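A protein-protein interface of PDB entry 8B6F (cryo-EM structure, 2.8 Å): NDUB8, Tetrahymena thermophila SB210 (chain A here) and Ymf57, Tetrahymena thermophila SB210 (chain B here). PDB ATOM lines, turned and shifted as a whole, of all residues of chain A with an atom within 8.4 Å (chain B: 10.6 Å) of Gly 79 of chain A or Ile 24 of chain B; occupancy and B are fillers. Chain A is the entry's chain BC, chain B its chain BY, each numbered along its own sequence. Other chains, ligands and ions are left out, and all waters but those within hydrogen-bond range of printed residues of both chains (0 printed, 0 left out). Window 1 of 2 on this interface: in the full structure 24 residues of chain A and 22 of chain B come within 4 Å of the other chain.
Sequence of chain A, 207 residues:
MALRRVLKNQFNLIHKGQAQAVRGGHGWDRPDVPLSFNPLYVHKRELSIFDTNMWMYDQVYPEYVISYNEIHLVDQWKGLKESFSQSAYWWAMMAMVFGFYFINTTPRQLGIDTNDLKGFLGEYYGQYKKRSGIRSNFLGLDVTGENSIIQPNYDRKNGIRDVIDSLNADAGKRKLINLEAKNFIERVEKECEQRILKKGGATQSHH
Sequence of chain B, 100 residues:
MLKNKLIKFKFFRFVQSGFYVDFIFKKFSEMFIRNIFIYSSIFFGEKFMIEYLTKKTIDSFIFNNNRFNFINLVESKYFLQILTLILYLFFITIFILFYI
The side-chain carboxylate (OE2) of Glu 70 of chain A sits close to the side-chain carboxylate (OD1) of Asp 22 of chain B, 3.2 Å away. NE2 of His 72 of chain A sits at hydrogen-bond distance from OH of Tyr 20 of chain B. The side-chain hydroxyl (OH) of Tyr 68 of chain A lies close to the side-chain carboxylate (OE1) of Glu 30 of chain B. The side-chain amide nitrogen of Gln 76 of chain A lies within hydrogen-bond range of the side-chain sulfur of Met 31 of chain B (3.1 Å). OG of Ser 83 of chain A sits at hydrogen-bond distance from O of Phe 19 of chain B (3.0 Å).
The backbone carbonyl oxygen of Phe 14 of chain B sits at hydrogen-bond distance from the backbone NH of Phe 19 of chain B (3.2 Å). OG of Ser 83 of chain A lies within hydrogen-bond range of O of Gly 79 of chain A, 2.7 Å away. The backbone carbonyl oxygen (O) of Glu 82 of chain A lies within hydrogen-bond range of the side-chain hydroxyl (OG) of Ser 85 of chain A (2.7 Å). The side-chain carboxylate of Asp 75 of chain A lies within hydrogen-bond range of the backbone NH of Lys 78 of chain A (2.9 Å).
Tyr 68 of chain A touches Phe 23 of chain B (CB to CE1, 3.8 Å). CB of Ser 17 of chain B touches OE2 of Glu 70 of chain A (3.9 Å). Tyr 20 of chain B touches Glu 70 of chain A. Leu 73 of chain A touches Phe 23 of chain B. Phe 28 of chain B touches Trp 77 of chain A. Ile 24 of chain B touches Gly 79 of chain A. Glu 82 of chain A touches Tyr 20 of chain B (CG to CE2, 3.5 Å). Ser 83 of chain A touches Phe 14 of chain B (CA to CE1, 3.8 Å). Tyr 20 of chain B touches Ser 83 of chain A.
Of chain B, only Phe 23 (3.9 Å) comes within 4 Å of Asp 75 of chain A. Gly 79 of chain A touches just one residue of chain B: Ile 24 (3.9 Å). Of chain B, only Phe 14, Phe 19, Tyr 20 and Ile 24 come within 4 Å of Ser 83 of chain A. Printed residues of chain A within 4 Å of Asp 22 of chain B: Glu 70 (3.2 Å). Ile 24 of chain B touches just these residues of chain A: Gly 79 (3.9 Å), Leu 80 (3.8 Å) and Ser 83 (3.7 Å). Of the printed residues of chain A, Lys 27 of chain B touches Tyr 68 and Gln 76. Printed residues of chain A within 4 Å of Phe 28 of chain B: Trp 77. Of the printed residues of chain A, Met 31 of chain B touches Gln 76. The nearest residue of chain B that does not touch Gly 79 of chain A is Tyr 20 of chain B (4.2 Å). The nearest residue of chain A that does not touch Ile 24 of chain B is Gln 76 of chain A (4.2 Å).
Of the 17 printed residues of chain B, 12 touch a printed residue of chain A. Of the 17 printed residues of chain A, 12 touch a printed residue of chain B. Printed residues of chain A that touch a printed residue of chain B: Tyr 68, Glu 70, His 72, Leu 73, Asp 75, Gln 76, Trp 77, Gly 79, Leu 80, Glu 82, Ser 83 and Gln 86. Hydrophobic or aromatic side chains of chain A that line the printed part of chain B: Tyr 68, His 72, Leu 73, Trp 77 and Leu 80. Among the printed residues, no Asp or Glu carboxylate lies within 4 Å of a Lys or Arg side-chain nitrogen of the other chain.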
ATOM      1  N   TYR A  68     -16.828 -28.873  30.284  1.00  0.00           N
ATOM      2  CA  TYR A  68     -17.486 -27.590  30.519  1.00  0.00           C
ATOM      3  C   TYR A  68     -17.152 -27.141  31.939  1.00  0.00           C
ATOM      4  O   TYR A  68     -17.889 -27.429  32.884  1.00  0.00           O
ATOM      5  CB  TYR A  68     -18.985 -27.706  30.305  1.00  0.00           C
ATOM      6  CG  TYR A  68     -19.349 -28.192  28.926  1.00  0.00           C
ATOM      7  CD1 TYR A  68     -19.054 -27.433  27.801  1.00  0.00           C
ATOM      8  CD2 TYR A  68     -19.988 -29.409  28.746  1.00  0.00           C
ATOM      9  CE1 TYR A  68     -19.383 -27.874  26.540  1.00  0.00           C
ATOM     10  CE2 TYR A  68     -20.321 -29.859  27.488  1.00  0.00           C
ATOM     11  CZ  TYR A  68     -20.014 -29.086  26.389  1.00  0.00           C
ATOM     12  OH  TYR A  68     -20.345 -29.531  25.135  1.00  0.00           O
ATOM     13  N   GLU A  70     -16.981 -23.945  32.941  1.00  0.00           N
ATOM     14  CA  GLU A  70     -17.872 -22.835  33.275  1.00  0.00           C
ATOM     15  C   GLU A  70     -19.322 -23.320  33.302  1.00  0.00           C
ATOM     16  O   GLU A  70     -20.192 -22.839  32.579  1.00  0.00           O
ATOM     17  CB  GLU A  70     -17.692 -21.692  32.284  1.00  0.00           C
ATOM     18  CG  GLU A  70     -16.267 -21.172  32.173  1.00  0.00           C
ATOM     19  CD  GLU A  70     -15.398 -22.020  31.264  1.00  0.00           C
ATOM     20  OE1 GLU A  70     -15.845 -23.115  30.862  1.00  0.00           O
ATOM     21  OE2 GLU A  70     -14.270 -21.591  30.945  1.00  0.00           O
ATOM     22  N   HIS A  72     -21.408 -23.121  35.819  1.00  0.00           N
ATOM     23  CA  HIS A  72     -22.334 -22.239  36.521  1.00  0.00           C
ATOM     24  C   HIS A  72     -23.246 -21.520  35.539  1.00  0.00           C
ATOM     25  O   HIS A  72     -24.362 -21.129  35.898  1.00  0.00           O
ATOM     26  CB  HIS A  72     -21.563 -21.239  37.384  1.00  0.00           C
ATOM     27  CG  HIS A  72     -20.641 -20.352  36.609  1.00  0.00           C
ATOM     28  ND1 HIS A  72     -19.406 -20.769  36.163  1.00  0.00           N
ATOM     29  CD2 HIS A  72     -20.769 -19.065  36.208  1.00  0.00           C
ATOM     30  CE1 HIS A  72     -18.817 -19.780  35.515  1.00  0.00           C
ATOM     31  NE2 HIS A  72     -19.622 -18.734  35.530  1.00  0.00           N
ATOM     32  N   LEU A  73     -22.790 -21.332  34.304  1.00  0.00           N
ATOM     33  CA  LEU A  73     -23.657 -20.887  33.223  1.00  0.00           C
ATOM     34  C   LEU A  73     -24.413 -22.095  32.687  1.00  0.00           C
ATOM     35  O   LEU A  73     -23.800 -23.072  32.246  1.00  0.00           O
ATOM     36  CB  LEU A  73     -22.832 -20.233  32.118  1.00  0.00           C
ATOM     37  CG  LEU A  73     -21.853 -19.153  32.582  1.00  0.00           C
ATOM     38  CD1 LEU A  73     -20.870 -18.831  31.480  1.00  0.00           C
ATOM     39  CD2 LEU A  73     -22.597 -17.905  33.020  1.00  0.00           C
ATOM     40  N   VAL A  74     -25.744 -22.037  32.730  1.00  0.00           N
ATOM     41  CA  VAL A  74     -26.545 -23.212  32.397  1.00  0.00           C
ATOM     42  C   VAL A  74     -26.321 -23.620  30.946  1.00  0.00           C
ATOM     43  O   VAL A  74     -26.136 -24.803  30.636  1.00  0.00           O
ATOM     44  CB  VAL A  74     -28.033 -22.946  32.686  1.00  0.00           C
ATOM     45  CG1 VAL A  74     -28.870 -24.179  32.376  1.00  0.00           C
ATOM     46  CG2 VAL A  74     -28.225 -22.521  34.136  1.00  0.00           C
ATOM     47  N   ASP A  75     -26.327 -22.650  30.035  1.00  0.00           N
ATOM     48  CA  ASP A  75     -26.199 -22.938  28.615  1.00  0.00           C
ATOM     49  C   ASP A  75     -25.448 -21.801  27.938  1.00  0.00           C
ATOM     50  O   ASP A  75     -25.149 -20.773  28.548  1.00  0.00           O
ATOM     51  CB  ASP A  75     -27.570 -23.154  27.965  1.00  0.00           C
ATOM     52  CG  ASP A  75     -28.525 -22.008  28.223  1.00  0.00           C
ATOM     53  OD1 ASP A  75     -28.312 -20.915  27.659  1.00  0.00           O
ATOM     54  OD2 ASP A  75     -29.493 -22.200  28.989  1.00  0.00           O
ATOM     55  N   GLN A  76     -25.143 -22.004  26.654  1.00  0.00           N
ATOM     56  CA  GLN A  76     -24.356 -21.019  25.918  1.00  0.00           C
ATOM     57  C   GLN A  76     -25.092 -19.690  25.811  1.00  0.00           C
ATOM     58  O   GLN A  76     -24.469 -18.624  25.862  1.00  0.00           O
ATOM     59  CB  GLN A  76     -24.000 -21.550  24.527  1.00  0.00           C
ATOM     60  CG  GLN A  76     -25.181 -21.903  23.628  1.00  0.00           C
ATOM     61  CD  GLN A  76     -25.739 -23.283  23.902  1.00  0.00           C
ATOM     62  OE1 GLN A  76     -25.433 -23.897  24.922  1.00  0.00           O
ATOM     63  NE2 GLN A  76     -26.557 -23.781  22.986  1.00  0.00           N
ATOM     64  N   TRP A  77     -26.416 -19.730  25.655  1.00  0.00           N
ATOM     65  CA  TRP A  77     -27.176 -18.492  25.512  1.00  0.00           C
ATOM     66  C   TRP A  77     -27.019 -17.617  26.747  1.00  0.00           C
ATOM     67  O   TRP A  77     -26.724 -16.420  26.641  1.00  0.00           O
ATOM     68  CB  TRP A  77     -28.649 -18.803  25.253  1.00  0.00           C
ATOM     69  CG  TRP A  77     -28.864 -19.763  24.131  1.00  0.00           C
ATOM     70  CD1 TRP A  77     -29.395 -21.016  24.217  1.00  0.00           C
ATOM     71  CD2 TRP A  77     -28.544 -19.556  22.751  1.00  0.00           C
ATOM     72  NE1 TRP A  77     -29.431 -21.599  22.973  1.00  0.00           N
ATOM     73  CE2 TRP A  77     -28.914 -20.722  22.057  1.00  0.00           C
ATOM     74  CE3 TRP A  77     -27.983 -18.493  22.036  1.00  0.00           C
ATOM     75  CZ2 TRP A  77     -28.742 -20.858  20.683  1.00  0.00           C
ATOM     76  CZ3 TRP A  77     -27.812 -18.630  20.671  1.00  0.00           C
ATOM     77  CH2 TRP A  77     -28.191 -19.804  20.008  1.00  0.00           C
ATOM     78  N   LYS A  78     -27.214 -18.194  27.932  1.00  0.00           N
ATOM     79  CA  LYS A  78     -26.915 -17.459  29.155  1.00  0.00           C
ATOM     80  C   LYS A  78     -25.441 -17.087  29.221  1.00  0.00           C
ATOM     81  O   LYS A  78     -25.085 -16.054  29.797  1.00  0.00           O
ATOM     82  CB  LYS A  78     -27.314 -18.282  30.378  1.00  0.00           C
ATOM     83  CG  LYS A  78     -28.796 -18.616  30.429  1.00  0.00           C
ATOM     84  CD  LYS A  78     -29.165 -19.349  31.712  1.00  0.00           C
ATOM     85  CE  LYS A  78     -29.102 -18.428  32.924  1.00  0.00           C
ATOM     86  NZ  LYS A  78     -29.546 -19.118  34.170  1.00  0.00           N
ATOM     87  N   GLY A  79     -24.572 -17.918  28.647  1.00  0.00           N
ATOM     88  CA  GLY A  79     -23.168 -17.558  28.557  1.00  0.00           C
ATOM     89  C   GLY A  79     -22.947 -16.311  27.723  1.00  0.00           C
ATOM     90  O   GLY A  79     -22.174 -15.428  28.101  1.00  0.00           O
ATOM     91  N   LEU A  80     -23.620 -16.223  26.573  1.00  0.00           N
ATOM     92  CA  LEU A  80     -23.526 -15.015  25.761  1.00  0.00           C
ATOM     93  C   LEU A  80     -24.044 -13.805  26.524  1.00  0.00           C
ATOM     94  O   LEU A  80     -23.423 -12.737  26.506  1.00  0.00           O
ATOM     95  CB  LEU A  80     -24.305 -15.195  24.460  1.00  0.00           C
ATOM     96  CG  LEU A  80     -23.676 -16.115  23.415  1.00  0.00           C
ATOM     97  CD1 LEU A  80     -24.706 -16.517  22.380  1.00  0.00           C
ATOM     98  CD2 LEU A  80     -22.497 -15.432  22.748  1.00  0.00           C
ATOM     99  N   LYS A  81     -25.181 -13.952  27.204  1.00  0.00           N
ATOM    100  CA  LYS A  81     -25.735 -12.837  27.962  1.00  0.00           C
ATOM    101  C   LYS A  81     -24.744 -12.361  29.017  1.00  0.00           C
ATOM    102  O   LYS A  81     -24.481 -11.161  29.145  1.00  0.00           O
ATOM    103  CB  LYS A  81     -27.057 -13.248  28.606  1.00  0.00           C
ATOM    104  CG  LYS A  81     -27.746 -12.130  29.372  1.00  0.00           C
ATOM    105  CD  LYS A  81     -29.034 -12.616  30.009  1.00  0.00           C
ATOM    106  CE  LYS A  81     -29.713 -11.501  30.782  1.00  0.00           C
ATOM    107  NZ  LYS A  81     -30.950 -11.963  31.472  1.00  0.00           N
ATOM    108  N   GLU A  82     -24.192 -13.296  29.790  1.00  0.00           N
ATOM    109  CA  GLU A  82     -23.232 -12.925  30.823  1.00  0.00           C
ATOM    110  C   GLU A  82     -21.989 -12.291  30.213  1.00  0.00           C
ATOM    111  O   GLU A  82     -21.461 -11.308  30.743  1.00  0.00           O
ATOM    112  CB  GLU A  82     -22.856 -14.155  31.648  1.00  0.00           C
ATOM    113  CG  GLU A  82     -22.066 -13.844  32.911  1.00  0.00           C
ATOM    114  CD  GLU A  82     -22.917 -13.208  33.993  1.00  0.00           C
ATOM    115  OE1 GLU A  82     -24.128 -13.011  33.762  1.00  0.00           O
ATOM    116  OE2 GLU A  82     -22.375 -12.909  35.078  1.00  0.00           O
ATOM    117  N   SER A  83     -21.500 -12.848  29.103  1.00  0.00           N
ATOM    118  CA  SER A  83     -20.295 -12.313  28.478  1.00  0.00           C
ATOM    119  C   SER A  83     -20.492 -10.866  28.047  1.00  0.00           C
ATOM    120  O   SER A  83     -19.639 -10.008  28.301  1.00  0.00           O
ATOM    121  CB  SER A  83     -19.906 -13.174  27.277  1.00  0.00           C
ATOM    122  OG  SER A  83     -19.656 -14.512  27.667  1.00  0.00           O
ATOM    123  N   PHE A  84     -21.613 -10.574  27.386  1.00  0.00           N
ATOM    124  CA  PHE A  84     -21.850  -9.210  26.931  1.00  0.00           C
ATOM    125  C   PHE A  84     -22.095  -8.265  28.100  1.00  0.00           C
ATOM    126  O   PHE A  84     -21.598  -7.134  28.102  1.00  0.00           O
ATOM    127  CB  PHE A  84     -23.022  -9.184  25.952  1.00  0.00           C
ATOM    128  CG  PHE A  84     -22.636  -9.535  24.545  1.00  0.00           C
ATOM    129  CD1 PHE A  84     -22.582 -10.856  24.136  1.00  0.00           C
ATOM    130  CD2 PHE A  84     -22.314  -8.544  23.635  1.00  0.00           C
ATOM    131  CE1 PHE A  84     -22.223 -11.181  22.842  1.00  0.00           C
ATOM    132  CE2 PHE A  84     -21.952  -8.861  22.340  1.00  0.00           C
ATOM    133  CZ  PHE A  84     -21.906 -10.182  21.944  1.00  0.00           C
ATOM    134  N   SER A  85     -22.860  -8.704  29.101  1.00  0.00           N
ATOM    135  CA  SER A  85     -23.125  -7.839  30.245  1.00  0.00           C
ATOM    136  C   SER A  85     -21.836  -7.459  30.959  1.00  0.00           C
ATOM    137  O   SER A  85     -21.663  -6.308  31.375  1.00  0.00           O
ATOM    138  CB  SER A  85     -24.084  -8.535  31.208  1.00  0.00           C
ATOM    139  OG  SER A  85     -23.523  -9.750  31.677  1.00  0.00           O
ATOM    140  N   GLN A  86     -20.919  -8.415  31.117  1.00  0.00           N
ATOM    141  CA  GLN A  86     -19.652  -8.137  31.783  1.00  0.00           C
ATOM    142  C   GLN A  86     -18.679  -7.393  30.880  1.00  0.00           C
ATOM    143  O   GLN A  86     -17.889  -6.580  31.367  1.00  0.00           O
ATOM    144  CB  GLN A  86     -19.019  -9.437  32.276  1.00  0.00           C
ATOM    145  CG  GLN A  86     -19.871 -10.206  33.269  1.00  0.00           C
ATOM    146  CD  GLN A  86     -20.130  -9.425  34.539  1.00  0.00           C
ATOM    147  OE1 GLN A  86     -19.505  -8.397  34.789  1.00  0.00           O
ATOM    148  NE2 GLN A  86     -21.056  -9.912  35.352  1.00  0.00           N
ATOM    149  N   PHE B  14     -15.398 -14.269  35.673  1.00  0.00           N
ATOM    150  CA  PHE B  14     -15.733 -14.039  34.273  1.00  0.00           C
ATOM    151  C   PHE B  14     -14.486 -13.715  33.461  1.00  0.00           C
ATOM    152  O   PHE B  14     -14.275 -14.270  32.378  1.00  0.00           O
ATOM    153  CB  PHE B  14     -16.748 -12.903  34.151  1.00  0.00           C
ATOM    154  CG  PHE B  14     -16.651 -12.154  32.854  1.00  0.00           C
ATOM    155  CD1 PHE B  14     -17.235 -12.655  31.706  1.00  0.00           C
ATOM    156  CD2 PHE B  14     -15.958 -10.959  32.781  1.00  0.00           C
ATOM    157  CE1 PHE B  14     -17.139 -11.972  30.511  1.00  0.00           C
ATOM    158  CE2 PHE B  14     -15.858 -10.271  31.589  1.00  0.00           C
ATOM    159  CZ  PHE B  14     -16.449 -10.779  30.453  1.00  0.00           C
ATOM    160  N   SER B  17     -11.995 -16.697  33.212  1.00  0.00           N
ATOM    161  CA  SER B  17     -12.430 -17.753  32.308  1.00  0.00           C
ATOM    162  C   SER B  17     -12.302 -17.364  30.845  1.00  0.00           C
ATOM    163  O   SER B  17     -12.900 -18.022  29.987  1.00  0.00           O
ATOM    164  CB  SER B  17     -13.879 -18.141  32.611  1.00  0.00           C
ATOM    165  OG  SER B  17     -14.019 -18.570  33.954  1.00  0.00           O
ATOM    166  N   GLY B  18     -11.542 -16.318  30.539  1.00  0.00           N
ATOM    167  CA  GLY B  18     -11.391 -15.894  29.159  1.00  0.00           C
ATOM    168  C   GLY B  18     -12.690 -15.435  28.535  1.00  0.00           C
ATOM    169  O   GLY B  18     -12.923 -15.681  27.345  1.00  0.00           O
ATOM    170  N   PHE B  19     -13.544 -14.772  29.313  1.00  0.00           N
ATOM    171  CA  PHE B  19     -14.796 -14.196  28.833  1.00  0.00           C
ATOM    172  C   PHE B  19     -15.802 -15.254  28.400  1.00  0.00           C
ATOM    173  O   PHE B  19     -16.723 -14.953  27.636  1.00  0.00           O
ATOM    174  CB  PHE B  19     -14.554 -13.221  27.676  1.00  0.00           C
ATOM    175  CG  PHE B  19     -13.774 -11.999  28.062  1.00  0.00           C
ATOM    176  CD1 PHE B  19     -12.469 -12.100  28.512  1.00  0.00           C
ATOM    177  CD2 PHE B  19     -14.338 -10.743  27.947  1.00  0.00           C
ATOM    178  CE1 PHE B  19     -11.749 -10.974  28.858  1.00  0.00           C
ATOM    179  CE2 PHE B  19     -13.626  -9.616  28.291  1.00  0.00           C
ATOM    180  CZ  PHE B  19     -12.328  -9.732  28.747  1.00  0.00           C
ATOM    181  N   TYR B  20     -15.654 -16.490  28.868  1.00  0.00           N
ATOM    182  CA  TYR B  20     -16.549 -17.592  28.532  1.00  0.00           C
ATOM    183  C   TYR B  20     -16.524 -17.941  27.049  1.00  0.00           C
ATOM    184  O   TYR B  20     -17.392 -18.685  26.580  1.00  0.00           O
ATOM    185  CB  TYR B  20     -17.988 -17.285  28.962  1.00  0.00           C
ATOM    186  CG  TYR B  20     -18.132 -16.928  30.422  1.00  0.00           C
ATOM    187  CD1 TYR B  20     -17.396 -17.587  31.397  1.00  0.00           C
ATOM    188  CD2 TYR B  20     -19.001 -15.923  30.825  1.00  0.00           C
ATOM    189  CE1 TYR B  20     -17.526 -17.263  32.732  1.00  0.00           C
ATOM    190  CE2 TYR B  20     -19.138 -15.591  32.157  1.00  0.00           C
ATOM    191  CZ  TYR B  20     -18.398 -16.264  33.105  1.00  0.00           C
ATOM    192  OH  TYR B  20     -18.533 -15.935  34.432  1.00  0.00           O
ATOM    193  N   VAL B  21     -15.555 -17.421  26.295  1.00  0.00           N
ATOM    194  CA  VAL B  21     -15.501 -17.694  24.862  1.00  0.00           C
ATOM    195  C   VAL B  21     -15.332 -19.187  24.612  1.00  0.00           C
ATOM    196  O   VAL B  21     -16.007 -19.768  23.753  1.00  0.00           O
ATOM    197  CB  VAL B  21     -14.369 -16.881  24.208  1.00  0.00           C
ATOM    198  CG1 VAL B  21     -14.265 -17.197  22.721  1.00  0.00           C
ATOM    199  CG2 VAL B  21     -14.592 -15.397  24.419  1.00  0.00           C
ATOM    200  N   ASP B  22     -14.430 -19.832  25.354  1.00  0.00           N
ATOM    201  CA  ASP B  22     -14.211 -21.262  25.168  1.00  0.00           C
ATOM    202  C   ASP B  22     -15.467 -22.060  25.492  1.00  0.00           C
ATOM    203  O   ASP B  22     -15.813 -23.005  24.774  1.00  0.00           O
ATOM    204  CB  ASP B  22     -13.039 -21.732  26.031  1.00  0.00           C
ATOM    205  CG  ASP B  22     -13.266 -21.486  27.510  1.00  0.00           C
ATOM    206  OD1 ASP B  22     -14.257 -20.810  27.859  1.00  0.00           O
ATOM    207  OD2 ASP B  22     -12.457 -21.974  28.327  1.00  0.00           O
ATOM    208  N   PHE B  23     -16.166 -21.695  26.567  1.00  0.00           N
ATOM    209  CA  PHE B  23     -17.389 -22.401  26.928  1.00  0.00           C
ATOM    210  C   PHE B  23     -18.433 -22.283  25.825  1.00  0.00           C
ATOM    211  O   PHE B  23     -19.054 -23.277  25.433  1.00  0.00           O
ATOM    212  CB  PHE B  23     -17.934 -21.848  28.246  1.00  0.00           C
ATOM    213  CG  PHE B  23     -19.229 -22.472  28.680  1.00  0.00           C
ATOM    214  CD1 PHE B  23     -19.235 -23.628  29.439  1.00  0.00           C
ATOM    215  CD2 PHE B  23     -20.439 -21.892  28.342  1.00  0.00           C
ATOM    216  CE1 PHE B  23     -20.423 -24.200  29.844  1.00  0.00           C
ATOM    217  CE2 PHE B  23     -21.630 -22.458  28.744  1.00  0.00           C
ATOM    218  CZ  PHE B  23     -21.622 -23.615  29.495  1.00  0.00           C
ATOM    219  N   ILE B  24     -18.641 -21.071  25.310  1.00  0.00           N
ATOM    220  CA  ILE B  24     -19.649 -20.868  24.273  1.00  0.00           C
ATOM    221  C   ILE B  24     -19.278 -21.642  23.016  1.00  0.00           C
ATOM    222  O   ILE B  24     -20.118 -22.315  22.408  1.00  0.00           O
ATOM    223  CB  ILE B  24     -19.821 -19.367  23.984  1.00  0.00           C
ATOM    224  CG1 ILE B  24     -20.280 -18.637  25.247  1.00  0.00           C
ATOM    225  CG2 ILE B  24     -20.823 -19.148  22.861  1.00  0.00           C
ATOM    226  CD1 ILE B  24     -20.165 -17.138  25.156  1.00  0.00           C
ATOM    227  N   PHE B  25     -18.011 -21.557  22.606  1.00  0.00           N
ATOM    228  CA  PHE B  25     -17.576 -22.261  21.403  1.00  0.00           C
ATOM    229  C   PHE B  25     -17.706 -23.768  21.569  1.00  0.00           C
ATOM    230  O   PHE B  25     -18.089 -24.472  20.629  1.00  0.00           O
ATOM    231  CB  PHE B  25     -16.132 -21.886  21.063  1.00  0.00           C
ATOM    232  CG  PHE B  25     -15.976 -20.511  20.463  1.00  0.00           C
ATOM    233  CD1 PHE B  25     -17.071 -19.678  20.274  1.00  0.00           C
ATOM    234  CD2 PHE B  25     -14.727 -20.060  20.075  1.00  0.00           C
ATOM    235  CE1 PHE B  25     -16.917 -18.422  19.717  1.00  0.00           C
ATOM    236  CE2 PHE B  25     -14.568 -18.806  19.518  1.00  0.00           C
ATOM    237  CZ  PHE B  25     -15.663 -17.986  19.339  1.00  0.00           C
ATOM    238  N   LYS B  26     -17.388 -24.283  22.757  1.00  0.00           N
ATOM    239  CA  LYS B  26     -17.507 -25.717  22.986  1.00  0.00           C
ATOM    240  C   LYS B  26     -18.962 -26.167  22.944  1.00  0.00           C
ATOM    241  O   LYS B  26     -19.268 -27.235  22.403  1.00  0.00           O
ATOM    242  CB  LYS B  26     -16.858 -26.087  24.320  1.00  0.00           C
ATOM    243  CG  LYS B  26     -15.334 -26.115  24.263  1.00  0.00           C
ATOM    244  CD  LYS B  26     -14.716 -26.628  25.554  1.00  0.00           C
ATOM    245  CE  LYS B  26     -14.942 -25.665  26.702  1.00  0.00           C
ATOM    246  NZ  LYS B  26     -14.202 -26.078  27.928  1.00  0.00           N
ATOM    247  N   LYS B  27     -19.876 -25.370  23.501  1.00  0.00           N
ATOM    248  CA  LYS B  27     -21.290 -25.720  23.427  1.00  0.00           C
ATOM    249  C   LYS B  27     -21.772 -25.749  21.982  1.00  0.00           C
ATOM    250  O   LYS B  27     -22.480 -26.674  21.570  1.00  0.00           O
ATOM    251  CB  LYS B  27     -22.119 -24.734  24.250  1.00  0.00           C
ATOM    252  CG  LYS B  27     -22.014 -24.929  25.753  1.00  0.00           C
ATOM    253  CD  LYS B  27     -22.705 -26.211  26.192  1.00  0.00           C
ATOM    254  CE  LYS B  27     -22.712 -26.348  27.705  1.00  0.00           C
ATOM    255  NZ  LYS B  27     -23.409 -27.585  28.150  1.00  0.00           N
ATOM    256  N   PHE B  28     -21.406 -24.736  21.196  1.00  0.00           N
ATOM    257  CA  PHE B  28     -21.822 -24.708  19.797  1.00  0.00           C
ATOM    258  C   PHE B  28     -21.193 -25.852  19.015  1.00  0.00           C
ATOM    259  O   PHE B  28     -21.833 -26.436  18.134  1.00  0.00           O
ATOM    260  CB  PHE B  28     -21.479 -23.361  19.162  1.00  0.00           C
ATOM    261  CG  PHE B  28     -22.468 -22.278  19.481  1.00  0.00           C
ATOM    262  CD1 PHE B  28     -23.730 -22.291  18.910  1.00  0.00           C
ATOM    263  CD2 PHE B  28     -22.142 -21.250  20.347  1.00  0.00           C
ATOM    264  CE1 PHE B  28     -24.646 -21.302  19.197  1.00  0.00           C
ATOM    265  CE2 PHE B  28     -23.056 -20.257  20.639  1.00  0.00           C
ATOM    266  CZ  PHE B  28     -24.310 -20.283  20.062  1.00  0.00           C
ATOM    267  N   SER B  29     -19.940 -26.186  19.324  1.00  0.00           N
ATOM    268  CA  SER B  29     -19.290 -27.310  18.660  1.00  0.00           C
ATOM    269  C   SER B  29     -19.983 -28.622  19.003  1.00  0.00           C
ATOM    270  O   SER B  29     -20.137 -29.495  18.142  1.00  0.00           O
ATOM    271  CB  SER B  29     -17.814 -27.368  19.049  1.00  0.00           C
ATOM    272  OG  SER B  29     -17.661 -27.804  20.388  1.00  0.00           O
ATOM    273  N   GLU B  30     -20.415 -28.780  20.256  1.00  0.00           N
ATOM    274  CA  GLU B  30     -21.177 -29.968  20.619  1.00  0.00           C
ATOM    275  C   GLU B  30     -22.472 -30.048  19.824  1.00  0.00           C
ATOM    276  O   GLU B  30     -22.828 -31.112  19.310  1.00  0.00           O
ATOM    277  CB  GLU B  30     -21.481 -29.969  22.116  1.00  0.00           C
ATOM    278  CG  GLU B  30     -22.209 -31.221  22.587  1.00  0.00           C
ATOM    279  CD  GLU B  30     -22.658 -31.131  24.029  1.00  0.00           C
ATOM    280  OE1 GLU B  30     -22.454 -30.066  24.649  1.00  0.00           O
ATOM    281  OE2 GLU B  30     -23.211 -32.123  24.545  1.00  0.00           O
ATOM    282  N   MET B  31     -23.184 -28.928  19.700  1.00  0.00           N
ATOM    283  CA  MET B  31     -24.402 -28.918  18.897  1.00  0.00           C
ATOM    284  C   MET B  31     -24.106 -29.357  17.470  1.00  0.00           C
ATOM    285  O   MET B  31     -24.810 -30.202  16.909  1.00  0.00           O
ATOM    286  CB  MET B  31     -25.025 -27.523  18.915  1.00  0.00           C
ATOM    287  CG  MET B  31     -25.608 -27.126  20.262  1.00  0.00           C
ATOM    288  SD  MET B  31     -26.085 -25.389  20.342  1.00  0.00           S
ATOM    289  CE  MET B  31     -27.194 -25.273  18.945  1.00  0.00           C
ATOM    290  N   PHE B  32     -23.068 -28.781  16.864  1.00  0.00           N
ATOM    291  CA  PHE B  32     -22.722 -29.135  15.493  1.00  0.00           C
ATOM    292  C   PHE B  32     -22.376 -30.616  15.382  1.00  0.00           C
ATOM    293  O   PHE B  32     -22.820 -31.297  14.450  1.00  0.00           O
ATOM    294  CB  PHE B  32     -21.554 -28.275  15.011  1.00  0.00           C
ATOM    295  CG  PHE B  32     -21.065 -28.633  13.635  1.00  0.00           C
ATOM    296  CD1 PHE B  32     -20.079 -29.590  13.460  1.00  0.00           C
ATOM    297  CD2 PHE B  32     -21.585 -28.000  12.519  1.00  0.00           C
ATOM    298  CE1 PHE B  32     -19.627 -29.915  12.196  1.00  0.00           C
ATOM    299  CE2 PHE B  32     -21.137 -28.320  11.252  1.00  0.00           C
ATOM    300  CZ  PHE B  32     -20.156 -29.279  11.090  1.00  0.00           C
